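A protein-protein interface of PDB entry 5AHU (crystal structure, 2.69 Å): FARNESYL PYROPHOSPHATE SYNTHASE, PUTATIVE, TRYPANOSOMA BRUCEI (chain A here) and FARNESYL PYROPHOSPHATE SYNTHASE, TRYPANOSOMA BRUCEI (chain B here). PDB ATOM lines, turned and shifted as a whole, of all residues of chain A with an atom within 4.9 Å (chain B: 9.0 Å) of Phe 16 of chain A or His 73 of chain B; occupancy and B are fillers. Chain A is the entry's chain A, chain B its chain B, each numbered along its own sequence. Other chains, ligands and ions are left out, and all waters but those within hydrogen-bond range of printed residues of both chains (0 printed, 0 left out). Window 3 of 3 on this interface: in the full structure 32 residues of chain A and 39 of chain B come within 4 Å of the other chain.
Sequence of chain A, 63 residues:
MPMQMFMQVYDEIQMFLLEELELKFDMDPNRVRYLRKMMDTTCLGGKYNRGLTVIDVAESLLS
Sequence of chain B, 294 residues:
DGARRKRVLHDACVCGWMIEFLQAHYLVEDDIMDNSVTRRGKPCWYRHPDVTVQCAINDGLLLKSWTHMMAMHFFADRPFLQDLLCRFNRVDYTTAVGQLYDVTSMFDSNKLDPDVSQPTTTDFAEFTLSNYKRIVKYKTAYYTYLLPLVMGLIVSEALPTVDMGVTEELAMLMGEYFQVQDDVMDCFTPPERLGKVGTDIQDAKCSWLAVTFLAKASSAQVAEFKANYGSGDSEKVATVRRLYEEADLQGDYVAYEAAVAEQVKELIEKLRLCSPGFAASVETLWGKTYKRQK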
ATOM      1  N   GLU A  12       6.813 -23.091  22.022  1.00  0.00           N
ATOM      2  CA  GLU A  12       5.812 -24.110  22.425  1.00  0.00           C
ATOM      3  C   GLU A  12       4.401 -23.808  21.978  1.00  0.00           C
ATOM      4  O   GLU A  12       3.725 -24.641  21.372  1.00  0.00           O
ATOM      5  CB  GLU A  12       5.683 -24.193  23.922  1.00  0.00           C
ATOM      6  CG  GLU A  12       6.603 -25.154  24.607  1.00  0.00           C
ATOM      7  CD  GLU A  12       6.344 -25.129  26.090  1.00  0.00           C
ATOM      8  OE1 GLU A  12       5.202 -25.501  26.481  1.00  0.00           O
ATOM      9  OE2 GLU A  12       7.274 -24.691  26.834  1.00  0.00           O
ATOM     10  N   ILE A  13       3.955 -22.616  22.350  1.00  0.00           N
ATOM     11  CA  ILE A  13       2.625 -22.173  22.025  1.00  0.00           C
ATOM     12  C   ILE A  13       2.459 -22.205  20.519  1.00  0.00           C
ATOM     13  O   ILE A  13       1.491 -22.762  20.014  1.00  0.00           O
ATOM     14  CB  ILE A  13       2.374 -20.751  22.532  1.00  0.00           C
ATOM     15  CG1 ILE A  13       2.325 -20.754  24.056  1.00  0.00           C
ATOM     16  CG2 ILE A  13       1.064 -20.217  21.966  1.00  0.00           C
ATOM     17  CD1 ILE A  13       2.473 -19.378  24.674  1.00  0.00           C
ATOM     18  N   GLN A  14       3.420 -21.609  19.815  1.00  0.00           N
ATOM     19  CA  GLN A  14       3.371 -21.567  18.369  1.00  0.00           C
ATOM     20  C   GLN A  14       3.280 -22.967  17.794  1.00  0.00           C
ATOM     21  O   GLN A  14       2.544 -23.198  16.842  1.00  0.00           O
ATOM     22  CB  GLN A  14       4.560 -20.847  17.790  1.00  0.00           C
ATOM     23  CG  GLN A  14       4.500 -20.827  16.284  1.00  0.00           C
ATOM     24  CD  GLN A  14       5.467 -19.846  15.699  1.00  0.00           C
ATOM     25  OE1 GLN A  14       6.655 -20.123  15.669  1.00  0.00           O
ATOM     26  NE2 GLN A  14       4.973 -18.695  15.231  1.00  0.00           N
ATOM     27  N   MET A  15       4.007 -23.897  18.403  1.00  0.00           N
ATOM     28  CA  MET A  15       4.012 -25.272  17.951  1.00  0.00           C
ATOM     29  C   MET A  15       2.644 -25.917  18.144  1.00  0.00           C
ATOM     30  O   MET A  15       2.113 -26.603  17.286  1.00  0.00           O
ATOM     31  CB  MET A  15       5.076 -26.072  18.709  1.00  0.00           C
ATOM     32  CG  MET A  15       5.018 -27.570  18.400  1.00  0.00           C
ATOM     33  SD  MET A  15       6.191 -28.601  19.305  1.00  0.00           S
ATOM     34  CE  MET A  15       5.290 -30.148  19.368  1.00  0.00           C
ATOM     35  N   PHE A  16       2.090 -25.700  19.310  1.00  0.00           N
ATOM     36  CA  PHE A  16       0.814 -26.281  19.647  1.00  0.00           C
ATOM     37  C   PHE A  16      -0.308 -25.780  18.707  1.00  0.00           C
ATOM     38  O   PHE A  16      -1.100 -26.566  18.175  1.00  0.00           O
ATOM     39  CB  PHE A  16       0.520 -26.003  21.117  1.00  0.00           C
ATOM     40  CG  PHE A  16      -0.923 -26.027  21.438  1.00  0.00           C
ATOM     41  CD1 PHE A  16      -1.595 -27.237  21.524  1.00  0.00           C
ATOM     42  CD2 PHE A  16      -1.623 -24.841  21.625  1.00  0.00           C
ATOM     43  CE1 PHE A  16      -2.948 -27.272  21.802  1.00  0.00           C
ATOM     44  CE2 PHE A  16      -2.960 -24.867  21.906  1.00  0.00           C
ATOM     45  CZ  PHE A  16      -3.626 -26.084  21.992  1.00  0.00           C
ATOM     46  N   LEU A  17      -0.327 -24.478  18.460  1.00  0.00           N
ATOM     47  CA  LEU A  17      -1.367 -23.856  17.646  1.00  0.00           C
ATOM     48  C   LEU A  17      -1.296 -24.274  16.201  1.00  0.00           C
ATOM     49  O   LEU A  17      -2.303 -24.581  15.603  1.00  0.00           O
ATOM     50  CB  LEU A  17      -1.289 -22.327  17.739  1.00  0.00           C
ATOM     51  CG  LEU A  17      -1.450 -21.769  19.157  1.00  0.00           C
ATOM     52  CD1 LEU A  17      -1.210 -20.261  19.130  1.00  0.00           C
ATOM     53  CD2 LEU A  17      -2.794 -22.114  19.795  1.00  0.00           C
ATOM     54  N   LEU A  18      -0.093 -24.273  15.647  1.00  0.00           N
ATOM     55  CA  LEU A  18       0.101 -24.611  14.246  1.00  0.00           C
ATOM     56  C   LEU A  18      -0.108 -26.077  13.952  1.00  0.00           C
ATOM     57  O   LEU A  18      -0.672 -26.431  12.919  1.00  0.00           O
ATOM     58  CB  LEU A  18       1.486 -24.193  13.815  1.00  0.00           C
ATOM     59  CG  LEU A  18       1.627 -22.682  13.868  1.00  0.00           C
ATOM     60  CD1 LEU A  18       3.029 -22.355  13.395  1.00  0.00           C
ATOM     61  CD2 LEU A  18       0.572 -21.969  13.029  1.00  0.00           C
ATOM     62  N   GLU A  19       0.352 -26.927  14.859  1.00  0.00           N
ATOM     63  CA  GLU A  19       0.128 -28.355  14.735  1.00  0.00           C
ATOM     64  C   GLU A  19      -1.338 -28.730  14.941  1.00  0.00           C
ATOM     65  O   GLU A  19      -1.906 -29.438  14.097  1.00  0.00           O
ATOM     66  CB  GLU A  19       1.050 -29.129  15.667  1.00  0.00           C
ATOM     67  CG  GLU A  19       2.386 -29.430  14.990  1.00  0.00           C
ATOM     68  CD  GLU A  19       3.478 -29.833  15.955  1.00  0.00           C
ATOM     69  OE1 GLU A  19       3.141 -30.504  16.961  1.00  0.00           O
ATOM     70  OE2 GLU A  19       4.659 -29.470  15.693  1.00  0.00           O
ATOM     71  N   GLU A  20      -1.954 -28.234  16.022  1.00  0.00           N
ATOM     72  CA  GLU A  20      -3.387 -28.409  16.235  1.00  0.00           C
ATOM     73  C   GLU A  20      -4.120 -28.053  14.955  1.00  0.00           C
ATOM     74  O   GLU A  20      -5.029 -28.746  14.553  1.00  0.00           O
ATOM     75  CB  GLU A  20      -3.882 -27.553  17.408  1.00  0.00           C
ATOM     76  CG  GLU A  20      -5.413 -27.547  17.606  1.00  0.00           C
ATOM     77  CD  GLU A  20      -5.927 -27.034  18.986  1.00  0.00           C
ATOM     78  OE1 GLU A  20      -5.767 -25.820  19.331  1.00  0.00           O
ATOM     79  OE2 GLU A  20      -6.561 -27.845  19.716  1.00  0.00           O
ATOM     80  N   LEU A  21      -3.696 -26.976  14.305  1.00  0.00           N
ATOM     81  CA  LEU A  21      -4.268 -26.552  13.031  1.00  0.00           C
ATOM     82  C   LEU A  21      -4.126 -27.608  11.969  1.00  0.00           C
ATOM     83  O   LEU A  21      -5.077 -27.897  11.284  1.00  0.00           O
ATOM     84  CB  LEU A  21      -3.642 -25.228  12.550  1.00  0.00           C
ATOM     85  CG  LEU A  21      -4.246 -24.014  13.256  1.00  0.00           C
ATOM     86  CD1 LEU A  21      -3.416 -22.778  12.980  1.00  0.00           C
ATOM     87  CD2 LEU A  21      -5.698 -23.770  12.843  1.00  0.00           C
ATOM     88  N   HIS B  10       6.062 -20.956  34.269  1.00  0.00           N
ATOM     89  CA  HIS B  10       5.531 -21.325  32.949  1.00  0.00           C
ATOM     90  C   HIS B  10       4.153 -20.722  32.659  1.00  0.00           C
ATOM     91  O   HIS B  10       3.891 -20.281  31.545  1.00  0.00           O
ATOM     92  CB  HIS B  10       5.471 -22.836  32.771  1.00  0.00           C
ATOM     93  CG  HIS B  10       5.331 -23.251  31.345  1.00  0.00           C
ATOM     94  ND1 HIS B  10       4.109 -23.424  30.739  1.00  0.00           N
ATOM     95  CD2 HIS B  10       6.262 -23.504  30.399  1.00  0.00           C
ATOM     96  CE1 HIS B  10       4.295 -23.797  29.486  1.00  0.00           C
ATOM     97  NE2 HIS B  10       5.594 -23.855  29.256  1.00  0.00           N
ATOM     98  N   ASP B  11       3.290 -20.715  33.666  1.00  0.00           N
ATOM     99  CA  ASP B  11       1.937 -20.182  33.543  1.00  0.00           C
ATOM    100  C   ASP B  11       1.977 -18.681  33.324  1.00  0.00           C
ATOM    101  O   ASP B  11       1.183 -18.116  32.565  1.00  0.00           O
ATOM    102  CB  ASP B  11       1.105 -20.487  34.813  1.00  0.00           C
ATOM    103  CG  ASP B  11       0.776 -21.986  34.974  1.00  0.00           C
ATOM    104  OD1 ASP B  11       0.990 -22.785  34.016  1.00  0.00           O
ATOM    105  OD2 ASP B  11       0.310 -22.357  36.070  1.00  0.00           O
ATOM    106  N   VAL B  14       2.795 -18.156  29.806  1.00  0.00           N
ATOM    107  CA  VAL B  14       1.619 -18.361  28.960  1.00  0.00           C
ATOM    108  C   VAL B  14       0.727 -17.123  29.041  1.00  0.00           C
ATOM    109  O   VAL B  14       0.408 -16.510  28.017  1.00  0.00           O
ATOM    110  CB  VAL B  14       0.871 -19.655  29.334  1.00  0.00           C
ATOM    111  CG1 VAL B  14      -0.507 -19.731  28.670  1.00  0.00           C
ATOM    112  CG2 VAL B  14       1.703 -20.861  28.943  1.00  0.00           C
ATOM    113  N   MET B  18      -0.700 -14.612  26.228  1.00  0.00           N
ATOM    114  CA  MET B  18      -2.098 -14.232  26.076  1.00  0.00           C
ATOM    115  C   MET B  18      -2.222 -12.734  25.868  1.00  0.00           C
ATOM    116  O   MET B  18      -2.895 -12.290  24.947  1.00  0.00           O
ATOM    117  CB  MET B  18      -2.892 -14.630  27.291  1.00  0.00           C
ATOM    118  CG  MET B  18      -3.225 -16.106  27.316  1.00  0.00           C
ATOM    119  SD  MET B  18      -4.032 -16.593  28.844  1.00  0.00           S
ATOM    120  CE  MET B  18      -5.583 -15.764  28.564  1.00  0.00           C
ATOM    121  N   SER B  65      -8.552 -15.327  19.093  1.00  0.00           N
ATOM    122  CA  SER B  65      -8.931 -16.696  19.426  1.00  0.00           C
ATOM    123  C   SER B  65      -7.785 -17.478  20.021  1.00  0.00           C
ATOM    124  O   SER B  65      -8.000 -18.288  20.905  1.00  0.00           O
ATOM    125  CB  SER B  65      -9.472 -17.436  18.214  1.00  0.00           C
ATOM    126  OG  SER B  65     -10.868 -17.322  18.186  1.00  0.00           O
ATOM    127  N   TRP B  66      -6.568 -17.237  19.539  1.00  0.00           N
ATOM    128  CA  TRP B  66      -5.416 -17.991  20.030  1.00  0.00           C
ATOM    129  C   TRP B  66      -5.195 -17.779  21.499  1.00  0.00           C
ATOM    130  O   TRP B  66      -4.789 -18.704  22.178  1.00  0.00           O
ATOM    131  CB  TRP B  66      -4.121 -17.703  19.242  1.00  0.00           C
ATOM    132  CG  TRP B  66      -4.101 -18.329  17.876  1.00  0.00           C
ATOM    133  CD1 TRP B  66      -4.769 -19.451  17.478  1.00  0.00           C
ATOM    134  CD2 TRP B  66      -3.378 -17.872  16.736  1.00  0.00           C
ATOM    135  NE1 TRP B  66      -4.527 -19.699  16.162  1.00  0.00           N
ATOM    136  CE2 TRP B  66      -3.659 -18.753  15.686  1.00  0.00           C
ATOM    137  CE3 TRP B  66      -2.489 -16.818  16.509  1.00  0.00           C
ATOM    138  CZ2 TRP B  66      -3.103 -18.604  14.419  1.00  0.00           C
ATOM    139  CZ3 TRP B  66      -1.938 -16.665  15.255  1.00  0.00           C
ATOM    140  CH2 TRP B  66      -2.252 -17.554  14.220  1.00  0.00           C
ATOM    141  N   THR B  67      -5.501 -16.590  22.000  1.00  0.00           N
ATOM    142  CA  THR B  67      -5.383 -16.331  23.436  1.00  0.00           C
ATOM    143  C   THR B  67      -6.244 -17.315  24.197  1.00  0.00           C
ATOM    144  O   THR B  67      -5.805 -17.858  25.202  1.00  0.00           O
ATOM    145  CB  THR B  67      -5.824 -14.900  23.848  1.00  0.00           C
ATOM    146  OG1 THR B  67      -7.227 -14.719  23.612  1.00  0.00           O
ATOM    147  CG2 THR B  67      -5.062 -13.836  23.078  1.00  0.00           C
ATOM    148  N   HIS B  68      -7.467 -17.540  23.717  1.00  0.00           N
ATOM    149  CA  HIS B  68      -8.360 -18.496  24.362  1.00  0.00           C
ATOM    150  C   HIS B  68      -7.906 -19.916  24.172  1.00  0.00           C
ATOM    151  O   HIS B  68      -8.036 -20.710  25.075  1.00  0.00           O
ATOM    152  CB  HIS B  68      -9.775 -18.348  23.839  1.00  0.00           C
ATOM    153  CG  HIS B  68     -10.373 -17.024  24.165  1.00  0.00           C
ATOM    154  ND1 HIS B  68     -10.974 -16.213  23.221  1.00  0.00           N
ATOM    155  CD2 HIS B  68     -10.398 -16.336  25.331  1.00  0.00           C
ATOM    156  CE1 HIS B  68     -11.375 -15.095  23.806  1.00  0.00           C
ATOM    157  NE2 HIS B  68     -11.037 -15.145  25.085  1.00  0.00           N
ATOM    158  N   MET B  69      -7.355 -20.241  23.007  1.00  0.00           N
ATOM    159  CA  MET B  69      -6.910 -21.609  22.746  1.00  0.00           C
ATOM    160  C   MET B  69      -5.700 -21.967  23.591  1.00  0.00           C
ATOM    161  O   MET B  69      -5.644 -23.062  24.145  1.00  0.00           O
ATOM    162  CB  MET B  69      -6.636 -21.839  21.261  1.00  0.00           C
ATOM    163  CG  MET B  69      -7.858 -21.597  20.379  1.00  0.00           C
ATOM    164  SD  MET B  69      -9.398 -22.390  20.950  1.00  0.00           S
ATOM    165  CE  MET B  69      -8.867 -24.051  20.538  1.00  0.00           C
ATOM    166  N   MET B  70      -4.751 -21.041  23.720  1.00  0.00           N
ATOM    167  CA  MET B  70      -3.564 -21.303  24.526  1.00  0.00           C
ATOM    168  C   MET B  70      -3.964 -21.415  25.994  1.00  0.00           C
ATOM    169  O   MET B  70      -3.546 -22.319  26.667  1.00  0.00           O
ATOM    170  CB  MET B  70      -2.431 -20.289  24.245  1.00  0.00           C
ATOM    171  CG  MET B  70      -2.602 -18.900  24.836  1.00  0.00           C
ATOM    172  SD  MET B  70      -1.204 -17.812  24.503  1.00  0.00           S
ATOM    173  CE  MET B  70      -1.604 -17.309  22.830  1.00  0.00           C
ATOM    174  N   ALA B  71      -4.834 -20.548  26.483  1.00  0.00           N
ATOM    175  CA  ALA B  71      -5.253 -20.616  27.894  1.00  0.00           C
ATOM    176  C   ALA B  71      -5.931 -21.948  28.227  1.00  0.00           C
ATOM    177  O   ALA B  71      -5.765 -22.485  29.319  1.00  0.00           O
ATOM    178  CB  ALA B  71      -6.180 -19.471  28.235  1.00  0.00           C
ATOM    179  N   MET B  72      -6.704 -22.467  27.281  1.00  0.00           N
ATOM    180  CA  MET B  72      -7.528 -23.625  27.537  1.00  0.00           C
ATOM    181  C   MET B  72      -6.619 -24.843  27.532  1.00  0.00           C
ATOM    182  O   MET B  72      -6.826 -25.807  28.278  1.00  0.00           O
ATOM    183  CB  MET B  72      -8.634 -23.731  26.482  1.00  0.00           C
ATOM    184  CG  MET B  72      -9.862 -24.498  26.950  1.00  0.00           C
ATOM    185  SD  MET B  72     -10.818 -23.717  28.301  1.00  0.00           S
ATOM    186  CE  MET B  72     -11.417 -22.226  27.501  1.00  0.00           C
ATOM    187  N   HIS B  73      -5.595 -24.786  26.687  1.00  0.00           N
ATOM    188  CA  HIS B  73      -4.653 -25.865  26.585  1.00  0.00           C
ATOM    189  C   HIS B  73      -3.875 -25.939  27.871  1.00  0.00           C
ATOM    190  O   HIS B  73      -3.908 -26.919  28.579  1.00  0.00           O
ATOM    191  CB  HIS B  73      -3.716 -25.630  25.429  1.00  0.00           C
ATOM    192  CG  HIS B  73      -2.804 -26.780  25.148  1.00  0.00           C
ATOM    193  ND1 HIS B  73      -1.436 -26.721  25.337  1.00  0.00           N
ATOM    194  CD2 HIS B  73      -3.066 -28.017  24.677  1.00  0.00           C
ATOM    195  CE1 HIS B  73      -0.898 -27.880  25.001  1.00  0.00           C
ATOM    196  NE2 HIS B  73      -1.868 -28.686  24.610  1.00  0.00           N
ATOM    197  N   PHE B  74      -3.205 -24.866  28.205  1.00  0.00           N
ATOM    198  CA  PHE B  74      -2.260 -24.924  29.285  1.00  0.00           C
ATOM    199  C   PHE B  74      -2.902 -24.916  30.669  1.00  0.00           C
ATOM    200  O   PHE B  74      -2.376 -25.523  31.594  1.00  0.00           O
ATOM    201  CB  PHE B  74      -1.253 -23.791  29.124  1.00  0.00           C
ATOM    202  CG  PHE B  74      -0.334 -23.992  27.968  1.00  0.00           C
ATOM    203  CD1 PHE B  74       0.644 -24.966  28.021  1.00  0.00           C
ATOM    204  CD2 PHE B  74      -0.472 -23.233  26.824  1.00  0.00           C
ATOM    205  CE1 PHE B  74       1.488 -25.166  26.960  1.00  0.00           C
ATOM    206  CE2 PHE B  74       0.369 -23.426  25.748  1.00  0.00           C
ATOM    207  CZ  PHE B  74       1.359 -24.401  25.815  1.00  0.00           C
ATOM    208  N   PHE B  75      -4.038 -24.249  30.800  1.00  0.00           N
ATOM    209  CA  PHE B  75      -4.662 -24.093  32.096  1.00  0.00           C
ATOM    210  C   PHE B  75      -5.877 -24.996  32.294  1.00  0.00           C
ATOM    211  O   PHE B  75      -6.577 -24.885  33.282  1.00  0.00           O
ATOM    212  CB  PHE B  75      -5.051 -22.634  32.318  1.00  0.00           C
ATOM    213  CG  PHE B  75      -3.913 -21.652  32.169  1.00  0.00           C
ATOM    214  CD1 PHE B  75      -2.614 -21.979  32.534  1.00  0.00           C
ATOM    215  CD2 PHE B  75      -4.167 -20.364  31.695  1.00  0.00           C
ATOM    216  CE1 PHE B  75      -1.592 -21.054  32.404  1.00  0.00           C
ATOM    217  CE2 PHE B  75      -3.150 -19.442  31.570  1.00  0.00           C
ATOM    218  CZ  PHE B  75      -1.859 -19.782  31.922  1.00  0.00           C
ATOM    219  N   ALA B  76      -6.114 -25.899  31.348  1.00  0.00           N
ATOM    220  CA  ALA B  76      -7.219 -26.856  31.408  1.00  0.00           C
ATOM    221  C   ALA B  76      -7.542 -27.326  32.834  1.00  0.00           C
ATOM    222  O   ALA B  76      -8.716 -27.315  33.243  1.00  0.00           O
ATOM    223  CB  ALA B  76      -6.887 -28.050  30.534  1.00  0.00           C
ATOM    224  N   ASP B  77      -6.501 -27.705  33.591  1.00  0.00           N
ATOM    225  CA  ASP B  77      -6.672 -28.337  34.903  1.00  0.00           C
ATOM    226  C   ASP B  77      -6.448 -27.490  36.129  1.00  0.00           C
ATOM    227  O   ASP B  77      -6.240 -27.975  37.229  1.00  0.00           O
ATOM    228  CB  ASP B  77      -5.948 -29.665  34.918  1.00  0.00           C
ATOM    229  CG  ASP B  77      -6.442 -30.598  33.822  1.00  0.00           C
ATOM    230  OD1 ASP B  77      -7.696 -30.718  33.617  1.00  0.00           O
ATOM    231  OD2 ASP B  77      -5.552 -31.193  33.164  1.00  0.00           O
ATOM    232  N   ARG B  78      -6.541 -26.198  35.926  1.00  0.00           N
ATOM    233  CA  ARG B  78      -6.151 -25.228  36.906  1.00  0.00           C
ATOM    234  C   ARG B  78      -7.351 -24.545  37.550  1.00  0.00           C
ATOM    235  O   ARG B  78      -8.274 -24.117  36.841  1.00  0.00           O
ATOM    236  CB  ARG B  78      -5.379 -24.265  36.024  1.00  0.00           C
ATOM    237  CG  ARG B  78      -4.203 -23.605  36.691  1.00  0.00           C
ATOM    238  CD  ARG B  78      -3.051 -24.568  36.991  1.00  0.00           C
ATOM    239  NE  ARG B  78      -1.942 -24.443  36.057  1.00  0.00           N
ATOM    240  CZ  ARG B  78      -1.161 -25.442  35.661  1.00  0.00           C
ATOM    241  NH1 ARG B  78      -1.384 -26.668  36.095  1.00  0.00           N
ATOM    242  NH2 ARG B  78      -0.173 -25.226  34.803  1.00  0.00           N
ATOM    243  N   LEU B  81      -8.538 -20.988  36.238  1.00  0.00           N
ATOM    244  CA  LEU B  81      -8.957 -20.809  34.851  1.00  0.00           C
ATOM    245  C   LEU B  81     -10.212 -20.003  34.692  1.00  0.00           C
ATOM    246  O   LEU B  81     -10.269 -19.127  33.865  1.00  0.00           O
ATOM    247  CB  LEU B  81      -9.215 -22.146  34.163  1.00  0.00           C
ATOM    248  CG  LEU B  81      -9.619 -22.081  32.681  1.00  0.00           C
ATOM    249  CD1 LEU B  81      -8.675 -21.237  31.844  1.00  0.00           C
ATOM    250  CD2 LEU B  81      -9.687 -23.471  32.086  1.00  0.00           C
ATOM    251  N   LEU B  85     -10.097 -16.130  32.942  1.00  0.00           N
ATOM    252  CA  LEU B  85     -10.830 -15.858  31.717  1.00  0.00           C
ATOM    253  C   LEU B  85     -11.895 -14.791  31.906  1.00  0.00           C
ATOM    254  O   LEU B  85     -12.123 -14.021  31.003  1.00  0.00           O
ATOM    255  CB  LEU B  85     -11.457 -17.152  31.164  1.00  0.00           C
ATOM    256  CG  LEU B  85     -10.473 -18.128  30.481  1.00  0.00           C
ATOM    257  CD1 LEU B  85     -11.184 -19.448  30.214  1.00  0.00           C
ATOM    258  CD2 LEU B  85      -9.836 -17.566  29.195  1.00  0.00           C
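Glu 12 of chain A touches Phe 74 of chain B (OE1 to CE1, 3.8 Å).
Phe 74 of chain B touches Ile 13 of chain A.
Met 69 of chain B touches Phe 16 of chain A.
Phe 16 of chain A touches His 73 of chain B.
Trp 66 of chain B touches Leu 17 of chain A.
Met 69 of chain B touches Glu 20 of chain A (CE to OE1, 3.8 Å).
Of the 10 printed residues of chain A, 5 touch a printed residue of chain B.
Among the printed residues, 7 pairs touch across the chains.
Among the printed residues, no Asp or Glu carboxylate lies within 4 Å of a Lys or Arg side-chain nitrogen of the other chain.
Printed residues of chain B within 4 Å of Ile 13 of chain A: Phe 74.
Phe 16 of chain A touches just these residues of chain B: Met 69 (3.9 Å) and His 73 (3.0 Å).
Of the printed residues of chain B, Leu 17 of chain A touches Trp 66.
Printed residues of chain B within 4 Å of Glu 20 of chain A: Met 69.
Of the printed residues of chain A, Trp 66 of chain B touches Leu 17.
Thr 67 of chain B touches none of the printed residues of chain A.
Of chain A, only Phe 16 comes within 4 Å of His 73 of chain B.
Printed residues of chain A within 4 Å of Phe 74 of chain B: Glu 12 (3.8 Å) and Ile 13 (3.7 Å).
Phe 75 of chain B touches none of the printed residues of chain A.
The nearest residue of chain B that does not touch Phe 16 of chain A is Met 70 of chain B (4.5 Å).
The nearest printed residue of chain B that does not touch Ile 13 of chain A is Met 70 of chain B (4.0002 Å).
OE2 of Glu 12 of chain A is in hydrogen-bond range of NE2 of His 10 of chain B (3.1 Å).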
